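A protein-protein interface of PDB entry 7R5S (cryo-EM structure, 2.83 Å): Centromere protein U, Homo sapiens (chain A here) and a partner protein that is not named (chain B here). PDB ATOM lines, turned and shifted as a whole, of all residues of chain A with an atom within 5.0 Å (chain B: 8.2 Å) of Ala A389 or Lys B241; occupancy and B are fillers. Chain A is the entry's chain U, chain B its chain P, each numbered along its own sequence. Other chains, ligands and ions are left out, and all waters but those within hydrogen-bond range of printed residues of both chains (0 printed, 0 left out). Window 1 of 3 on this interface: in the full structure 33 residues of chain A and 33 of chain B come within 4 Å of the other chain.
Among the printed residues, merely in contact across the chains: Tyr A382 with Lys B241 (3.6 Å), Tyr A382 with Val B242 (3.8 Å), Tyr A382 with Pro B243 (3.8 Å), Tyr A382 with Gln B244 (3.8 Å), Ser A386 with Lys B241 (3.6 Å), Pro A388 with Leu B239 (3.3 Å), Ala A389 with Leu B239 (3.6 Å), Ala A389 with Lys B241 (3.6 Å), Leu A390 with Lys B241 (3.7 Å), Phe A392 with Val B221 (3.5 Å), Phe A392 with Leu B239 (3.7 Å) and Lys A393 with Arg B209 (3.96 Å).
Of the 17 printed residues of chain B, 9 touch a printed residue of chain A.
Printed residues of chain A that touch a printed residue of chain B: Tyr A382, Ser A386, Pro A388, Ala A389, Leu A390, Phe A392 and Lys A393.
Among the printed residues, Asp or Glu carboxylates within 4 Å of a Lys or Arg side-chain nitrogen of the other chain: Lys A393 with Glu B217 (2.6 Å).
Lys B241 touches just these residues of chain A: Tyr A382 (3.6 Å), Ser A386 (3.6 Å), Ala A389 (3.6 Å), Leu A390 (3.7 Å) and Lys A393 (3.2 Å).
Pro A388 touches just one residue of chain B: Leu B239.
Of the printed residues of chain B, Lys A393 touches Arg B209, Glu B217 and Lys B241.
Printed residues of chain B within 4 Å of Tyr A382: Lys B241, Val B242, Pro B243 and Gln B244.
Printed residues of chain A within 4 Å of Val B242: Tyr A382 and Ser A386.
The nearest printed residue of chain B that does not touch Ser A386 is Pro B243 (5.1 Å).
The backbone carbonyl oxygen (O) of Val B219 is in hydrogen-bond range of the backbone NH (N) of Leu B239 (3.1 Å).
The side-chain amino group (NZ) of Lys B241 is in salt-bridge range of the side-chain carboxylate (OE1) of Glu B217, at 3.7 Å.
The backbone NH of Val B242 is in hydrogen-bond range of the side-chain hydroxyl of Ser A386, at 3.2 Å.
The side-chain amino group (NZ) of Lys A393 is in salt-bridge range of the side-chain carboxylate (OE1) of Glu B217 (2.6 Å).
OG of Ser A386 sits close to O of Thr B240.
NZ of Lys A393 lies close to NZ of Lys B241, 3.2 Å away.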
ATOM      1  N   TYR A 382      18.698   7.450  -9.053  1.00  0.00           N
ATOM      2  CA  TYR A 382      18.786   7.990  -7.706  1.00  0.00           C
ATOM      3  C   TYR A 382      18.919   6.857  -6.698  1.00  0.00           C
ATOM      4  O   TYR A 382      18.439   5.742  -6.921  1.00  0.00           O
ATOM      5  CB  TYR A 382      17.564   8.856  -7.371  1.00  0.00           C
ATOM      6  CG  TYR A 382      17.480  10.128  -8.187  1.00  0.00           C
ATOM      7  CD1 TYR A 382      18.127  11.286  -7.774  1.00  0.00           C
ATOM      8  CD2 TYR A 382      16.755  10.170  -9.371  1.00  0.00           C
ATOM      9  CE1 TYR A 382      18.054  12.450  -8.518  1.00  0.00           C
ATOM     10  CE2 TYR A 382      16.676  11.329 -10.121  1.00  0.00           C
ATOM     11  CZ  TYR A 382      17.328  12.465  -9.690  1.00  0.00           C
ATOM     12  OH  TYR A 382      17.252  13.621 -10.433  1.00  0.00           O
ATOM     13  N   SER A 386      17.679   9.452  -1.428  1.00  0.00           N
ATOM     14  CA  SER A 386      17.023  10.585  -2.066  1.00  0.00           C
ATOM     15  C   SER A 386      15.503  10.541  -1.955  1.00  0.00           C
ATOM     16  O   SER A 386      14.840  11.503  -2.353  1.00  0.00           O
ATOM     17  CB  SER A 386      17.424  10.662  -3.543  1.00  0.00           C
ATOM     18  OG  SER A 386      18.827  10.824  -3.677  1.00  0.00           O
ATOM     19  N   LEU A 387      14.941   9.463  -1.417  1.00  0.00           N
ATOM     20  CA  LEU A 387      13.493   9.327  -1.288  1.00  0.00           C
ATOM     21  C   LEU A 387      12.869  10.312  -0.301  1.00  0.00           C
ATOM     22  O   LEU A 387      11.727  10.732  -0.518  1.00  0.00           O
ATOM     23  CB  LEU A 387      13.111   7.898  -0.899  1.00  0.00           C
ATOM     24  CG  LEU A 387      13.098   6.850  -2.016  1.00  0.00           C
ATOM     25  CD1 LEU A 387      14.480   6.540  -2.578  1.00  0.00           C
ATOM     26  CD2 LEU A 387      12.413   5.590  -1.530  1.00  0.00           C
ATOM     27  N   PRO A 388      13.533  10.681   0.803  1.00  0.00           N
ATOM     28  CA  PRO A 388      12.963  11.754   1.638  1.00  0.00           C
ATOM     29  C   PRO A 388      12.767  13.062   0.888  1.00  0.00           C
ATOM     30  O   PRO A 388      11.698  13.678   0.993  1.00  0.00           O
ATOM     31  CB  PRO A 388      13.986  11.889   2.772  1.00  0.00           C
ATOM     32  CG  PRO A 388      14.558  10.536   2.899  1.00  0.00           C
ATOM     33  CD  PRO A 388      14.639   9.995   1.501  1.00  0.00           C
ATOM     34  N   ALA A 389      13.769  13.503   0.123  1.00  0.00           N
ATOM     35  CA  ALA A 389      13.620  14.742  -0.633  1.00  0.00           C
ATOM     36  C   ALA A 389      12.594  14.586  -1.748  1.00  0.00           C
ATOM     37  O   ALA A 389      11.861  15.531  -2.063  1.00  0.00           O
ATOM     38  CB  ALA A 389      14.969  15.180  -1.199  1.00  0.00           C
ATOM     39  N   LEU A 390      12.515  13.396  -2.347  1.00  0.00           N
ATOM     40  CA  LEU A 390      11.496  13.147  -3.363  1.00  0.00           C
ATOM     41  C   LEU A 390      10.097  13.228  -2.765  1.00  0.00           C
ATOM     42  O   LEU A 390       9.177  13.777  -3.384  1.00  0.00           O
ATOM     43  CB  LEU A 390      11.729  11.780  -4.005  1.00  0.00           C
ATOM     44  CG  LEU A 390      12.916  11.658  -4.965  1.00  0.00           C
ATOM     45  CD1 LEU A 390      13.142  10.208  -5.364  1.00  0.00           C
ATOM     46  CD2 LEU A 390      12.718  12.528  -6.194  1.00  0.00           C
ATOM     47  N   LEU A 391       9.922  12.699  -1.553  1.00  0.00           N
ATOM     48  CA  LEU A 391       8.626  12.775  -0.889  1.00  0.00           C
ATOM     49  C   LEU A 391       8.298  14.205  -0.484  1.00  0.00           C
ATOM     50  O   LEU A 391       7.141  14.628  -0.566  1.00  0.00           O
ATOM     51  CB  LEU A 391       8.602  11.852   0.329  1.00  0.00           C
ATOM     52  CG  LEU A 391       7.920  10.496   0.132  1.00  0.00           C
ATOM     53  CD1 LEU A 391       7.883   9.716   1.438  1.00  0.00           C
ATOM     54  CD2 LEU A 391       6.518  10.676  -0.430  1.00  0.00           C
ATOM     55  N   PHE A 392       9.300  14.972  -0.056  1.00  0.00           N
ATOM     56  CA  PHE A 392       9.042  16.372   0.260  1.00  0.00           C
ATOM     57  C   PHE A 392       8.781  17.206  -0.988  1.00  0.00           C
ATOM     58  O   PHE A 392       8.164  18.272  -0.890  1.00  0.00           O
ATOM     59  CB  PHE A 392      10.199  16.967   1.060  1.00  0.00           C
ATOM     60  CG  PHE A 392       9.846  17.266   2.487  1.00  0.00           C
ATOM     61  CD1 PHE A 392       9.546  16.241   3.368  1.00  0.00           C
ATOM     62  CD2 PHE A 392       9.784  18.573   2.941  1.00  0.00           C
ATOM     63  CE1 PHE A 392       9.213  16.512   4.681  1.00  0.00           C
ATOM     64  CE2 PHE A 392       9.446  18.851   4.252  1.00  0.00           C
ATOM     65  CZ  PHE A 392       9.162  17.818   5.124  1.00  0.00           C
ATOM     66  N   LYS A 393       9.242  16.751  -2.155  1.00  0.00           N
ATOM     67  CA  LYS A 393       8.879  17.410  -3.405  1.00  0.00           C
ATOM     68  C   LYS A 393       7.468  17.029  -3.841  1.00  0.00           C
ATOM     69  O   LYS A 393       6.738  17.862  -4.388  1.00  0.00           O
ATOM     70  CB  LYS A 393       9.888  17.060  -4.498  1.00  0.00           C
ATOM     71  CG  LYS A 393      11.144  17.915  -4.483  1.00  0.00           C
ATOM     72  CD  LYS A 393      11.976  17.688  -5.734  1.00  0.00           C
ATOM     73  CE  LYS A 393      13.100  18.705  -5.845  1.00  0.00           C
ATOM     74  NZ  LYS A 393      13.883  18.526  -7.100  1.00  0.00           N
ATOM     75  N   ILE B 208      17.302  24.397  -2.456  1.00  0.00           N
ATOM     76  CA  ILE B 208      18.552  24.986  -2.916  1.00  0.00           C
ATOM     77  C   ILE B 208      19.021  24.218  -4.146  1.00  0.00           C
ATOM     78  O   ILE B 208      19.101  22.980  -4.135  1.00  0.00           O
ATOM     79  CB  ILE B 208      19.617  24.994  -1.805  1.00  0.00           C
ATOM     80  CG1 ILE B 208      20.942  25.550  -2.335  1.00  0.00           C
ATOM     81  CG2 ILE B 208      19.780  23.619  -1.185  1.00  0.00           C
ATOM     82  CD1 ILE B 208      21.844  26.101  -1.257  1.00  0.00           C
ATOM     83  N   ARG B 209      19.310  24.960  -5.214  1.00  0.00           N
ATOM     84  CA  ARG B 209      19.630  24.393  -6.513  1.00  0.00           C
ATOM     85  C   ARG B 209      20.424  25.417  -7.311  1.00  0.00           C
ATOM     86  O   ARG B 209      20.162  26.618  -7.219  1.00  0.00           O
ATOM     87  CB  ARG B 209      18.357  23.999  -7.272  1.00  0.00           C
ATOM     88  CG  ARG B 209      18.590  23.491  -8.686  1.00  0.00           C
ATOM     89  CD  ARG B 209      17.320  23.574  -9.514  1.00  0.00           C
ATOM     90  NE  ARG B 209      16.218  22.847  -8.891  1.00  0.00           N
ATOM     91  CZ  ARG B 209      14.981  22.809  -9.375  1.00  0.00           C
ATOM     92  NH1 ARG B 209      14.683  23.458 -10.491  1.00  0.00           N
ATOM     93  NH2 ARG B 209      14.041  22.122  -8.741  1.00  0.00           N
ATOM     94  N   PRO B 214      20.396  20.924 -13.068  1.00  0.00           N
ATOM     95  CA  PRO B 214      19.216  20.658 -12.235  1.00  0.00           C
ATOM     96  C   PRO B 214      19.240  19.312 -11.531  1.00  0.00           C
ATOM     97  O   PRO B 214      18.263  18.972 -10.854  1.00  0.00           O
ATOM     98  CB  PRO B 214      18.067  20.724 -13.250  1.00  0.00           C
ATOM     99  CG  PRO B 214      18.687  20.282 -14.530  1.00  0.00           C
ATOM    100  CD  PRO B 214      20.105  20.792 -14.506  1.00  0.00           C
ATOM    101  N   GLY B 215      20.316  18.539 -11.665  1.00  0.00           N
ATOM    102  CA  GLY B 215      20.397  17.239 -11.030  1.00  0.00           C
ATOM    103  C   GLY B 215      20.882  17.296  -9.597  1.00  0.00           C
ATOM    104  O   GLY B 215      20.327  16.626  -8.722  1.00  0.00           O
ATOM    105  N   PHE B 216      21.917  18.093  -9.342  1.00  0.00           N
ATOM    106  CA  PHE B 216      22.485  18.232  -8.001  1.00  0.00           C
ATOM    107  C   PHE B 216      21.774  19.383  -7.298  1.00  0.00           C
ATOM    108  O   PHE B 216      22.066  20.555  -7.547  1.00  0.00           O
ATOM    109  CB  PHE B 216      23.990  18.459  -8.068  1.00  0.00           C
ATOM    110  CG  PHE B 216      24.724  18.027  -6.828  1.00  0.00           C
ATOM    111  CD1 PHE B 216      25.582  16.940  -6.860  1.00  0.00           C
ATOM    112  CD2 PHE B 216      24.554  18.704  -5.632  1.00  0.00           C
ATOM    113  CE1 PHE B 216      26.259  16.539  -5.723  1.00  0.00           C
ATOM    114  CE2 PHE B 216      25.227  18.308  -4.493  1.00  0.00           C
ATOM    115  CZ  PHE B 216      26.080  17.225  -4.539  1.00  0.00           C
ATOM    116  N   GLU B 217      20.839  19.042  -6.416  1.00  0.00           N
ATOM    117  CA  GLU B 217      20.091  20.030  -5.654  1.00  0.00           C
ATOM    118  C   GLU B 217      19.509  19.344  -4.429  1.00  0.00           C
ATOM    119  O   GLU B 217      19.247  18.139  -4.449  1.00  0.00           O
ATOM    120  CB  GLU B 217      18.980  20.666  -6.494  1.00  0.00           C
ATOM    121  CG  GLU B 217      18.063  19.671  -7.186  1.00  0.00           C
ATOM    122  CD  GLU B 217      16.881  19.272  -6.325  1.00  0.00           C
ATOM    123  OE1 GLU B 217      16.393  18.134  -6.474  1.00  0.00           O
ATOM    124  OE2 GLU B 217      16.439  20.100  -5.500  1.00  0.00           O
ATOM    125  N   LEU B 218      19.307  20.117  -3.365  1.00  0.00           N
ATOM    126  CA  LEU B 218      18.804  19.542  -2.124  1.00  0.00           C
ATOM    127  C   LEU B 218      17.751  20.460  -1.519  1.00  0.00           C
ATOM    128  O   LEU B 218      17.438  21.527  -2.053  1.00  0.00           O
ATOM    129  CB  LEU B 218      19.934  19.260  -1.120  1.00  0.00           C
ATOM    130  CG  LEU B 218      20.970  20.337  -0.787  1.00  0.00           C
ATOM    131  CD1 LEU B 218      21.511  20.127   0.617  1.00  0.00           C
ATOM    132  CD2 LEU B 218      22.109  20.332  -1.794  1.00  0.00           C
ATOM    133  N   VAL B 219      17.183  20.013  -0.402  1.00  0.00           N
ATOM    134  CA  VAL B 219      16.106  20.723   0.276  1.00  0.00           C
ATOM    135  C   VAL B 219      16.450  20.867   1.752  1.00  0.00           C
ATOM    136  O   VAL B 219      17.067  19.980   2.353  1.00  0.00           O
ATOM    137  CB  VAL B 219      14.745  20.015   0.094  1.00  0.00           C
ATOM    138  CG1 VAL B 219      14.438  19.812  -1.383  1.00  0.00           C
ATOM    139  CG2 VAL B 219      14.723  18.681   0.822  1.00  0.00           C
ATOM    140  N   ILE B 220      16.073  22.007   2.318  1.00  0.00           N
ATOM    141  CA  ILE B 220      16.166  22.276   3.747  1.00  0.00           C
ATOM    142  C   ILE B 220      14.751  22.403   4.292  1.00  0.00           C
ATOM    143  O   ILE B 220      13.890  23.041   3.673  1.00  0.00           O
ATOM    144  CB  ILE B 220      16.990  23.548   4.029  1.00  0.00           C
ATOM    145  CG1 ILE B 220      18.387  23.417   3.421  1.00  0.00           C
ATOM    146  CG2 ILE B 220      17.084  23.806   5.525  1.00  0.00           C
ATOM    147  CD1 ILE B 220      19.240  24.654   3.575  1.00  0.00           C
ATOM    148  N   VAL B 221      14.511  21.789   5.448  1.00  0.00           N
ATOM    149  CA  VAL B 221      13.184  21.707   6.046  1.00  0.00           C
ATOM    150  C   VAL B 221      13.182  22.515   7.335  1.00  0.00           C
ATOM    151  O   VAL B 221      14.068  22.350   8.179  1.00  0.00           O
ATOM    152  CB  VAL B 221      12.778  20.247   6.316  1.00  0.00           C
ATOM    153  CG1 VAL B 221      11.417  20.189   6.986  1.00  0.00           C
ATOM    154  CG2 VAL B 221      12.787  19.445   5.024  1.00  0.00           C
ATOM    155  N   LEU B 238      17.520  18.472   6.774  1.00  0.00           N
ATOM    156  CA  LEU B 238      17.683  18.576   5.332  1.00  0.00           C
ATOM    157  C   LEU B 238      17.617  17.185   4.719  1.00  0.00           C
ATOM    158  O   LEU B 238      17.971  16.189   5.354  1.00  0.00           O
ATOM    159  CB  LEU B 238      18.996  19.276   4.943  1.00  0.00           C
ATOM    160  CG  LEU B 238      20.376  18.742   5.346  1.00  0.00           C
ATOM    161  CD1 LEU B 238      20.839  17.576   4.480  1.00  0.00           C
ATOM    162  CD2 LEU B 238      21.386  19.872   5.270  1.00  0.00           C
ATOM    163  N   LEU B 239      17.158  17.136   3.471  1.00  0.00           N
ATOM    164  CA  LEU B 239      17.073  15.904   2.704  1.00  0.00           C
ATOM    165  C   LEU B 239      17.829  16.093   1.398  1.00  0.00           C
ATOM    166  O   LEU B 239      17.709  17.136   0.749  1.00  0.00           O
ATOM    167  CB  LEU B 239      15.613  15.524   2.433  1.00  0.00           C
ATOM    168  CG  LEU B 239      14.662  15.735   3.614  1.00  0.00           C
ATOM    169  CD1 LEU B 239      13.212  15.574   3.191  1.00  0.00           C
ATOM    170  CD2 LEU B 239      14.998  14.789   4.758  1.00  0.00           C
ATOM    171  N   THR B 240      18.607  15.086   1.016  1.00  0.00           N
ATOM    172  CA  THR B 240      19.518  15.182  -0.119  1.00  0.00           C
ATOM    173  C   THR B 240      18.992  14.336  -1.270  1.00  0.00           C
ATOM    174  O   THR B 240      18.908  13.109  -1.156  1.00  0.00           O
ATOM    175  CB  THR B 240      20.927  14.730   0.271  1.00  0.00           C
ATOM    176  OG1 THR B 240      20.846  13.542   1.067  1.00  0.00           O
ATOM    177  CG2 THR B 240      21.632  15.820   1.064  1.00  0.00           C
ATOM    178  N   LYS B 241      18.645  14.993  -2.373  1.00  0.00           N
ATOM    179  CA  LYS B 241      18.247  14.326  -3.611  1.00  0.00           C
ATOM    180  C   LYS B 241      19.410  14.473  -4.588  1.00  0.00           C
ATOM    181  O   LYS B 241      19.472  15.425  -5.369  1.00  0.00           O
ATOM    182  CB  LYS B 241      16.957  14.914  -4.176  1.00  0.00           C
ATOM    183  CG  LYS B 241      16.507  14.271  -5.479  1.00  0.00           C
ATOM    184  CD  LYS B 241      15.440  15.101  -6.170  1.00  0.00           C
ATOM    185  CE  LYS B 241      15.303  14.714  -7.634  1.00  0.00           C
ATOM    186  NZ  LYS B 241      14.415  15.649  -8.375  1.00  0.00           N
ATOM    187  N   VAL B 242      20.339  13.525  -4.532  1.00  0.00           N
ATOM    188  CA  VAL B 242      21.530  13.558  -5.374  1.00  0.00           C
ATOM    189  C   VAL B 242      21.561  12.296  -6.229  1.00  0.00           C
ATOM    190  O   VAL B 242      21.337  11.192  -5.712  1.00  0.00           O
ATOM    191  CB  VAL B 242      22.804  13.706  -4.526  1.00  0.00           C
ATOM    192  CG1 VAL B 242      22.800  12.713  -3.370  1.00  0.00           C
ATOM    193  CG2 VAL B 242      24.044  13.530  -5.384  1.00  0.00           C
ATOM    194  N   PRO B 243      21.805  12.410  -7.535  1.00  0.00           N
ATOM    195  CA  PRO B 243      21.842  11.217  -8.386  1.00  0.00           C
ATOM    196  C   PRO B 243      22.962  10.269  -7.984  1.00  0.00           C
ATOM    197  O   PRO B 243      23.910  10.637  -7.286  1.00  0.00           O
ATOM    198  CB  PRO B 243      22.075  11.787  -9.791  1.00  0.00           C
ATOM    199  CG  PRO B 243      21.597  13.199  -9.710  1.00  0.00           C
ATOM    200  CD  PRO B 243      21.921  13.651  -8.319  1.00  0.00           C
ATOM    201  N   GLN B 244      22.838   9.022  -8.442  1.00  0.00           N
ATOM    202  CA  GLN B 244      23.824   7.996  -8.127  1.00  0.00           C
ATOM    203  C   GLN B 244      25.165   8.235  -8.810  1.00  0.00           C
ATOM    204  O   GLN B 244      26.135   7.540  -8.489  1.00  0.00           O
ATOM    205  CB  GLN B 244      23.282   6.617  -8.511  1.00  0.00           C
ATOM    206  CG  GLN B 244      23.869   5.467  -7.708  1.00  0.00           C
ATOM    207  CD  GLN B 244      22.845   4.396  -7.389  1.00  0.00           C
ATOM    208  OE1 GLN B 244      21.804   4.300  -8.040  1.00  0.00           O
ATOM    209  NE2 GLN B 244      23.135   3.582  -6.380  1.00  0.00           N
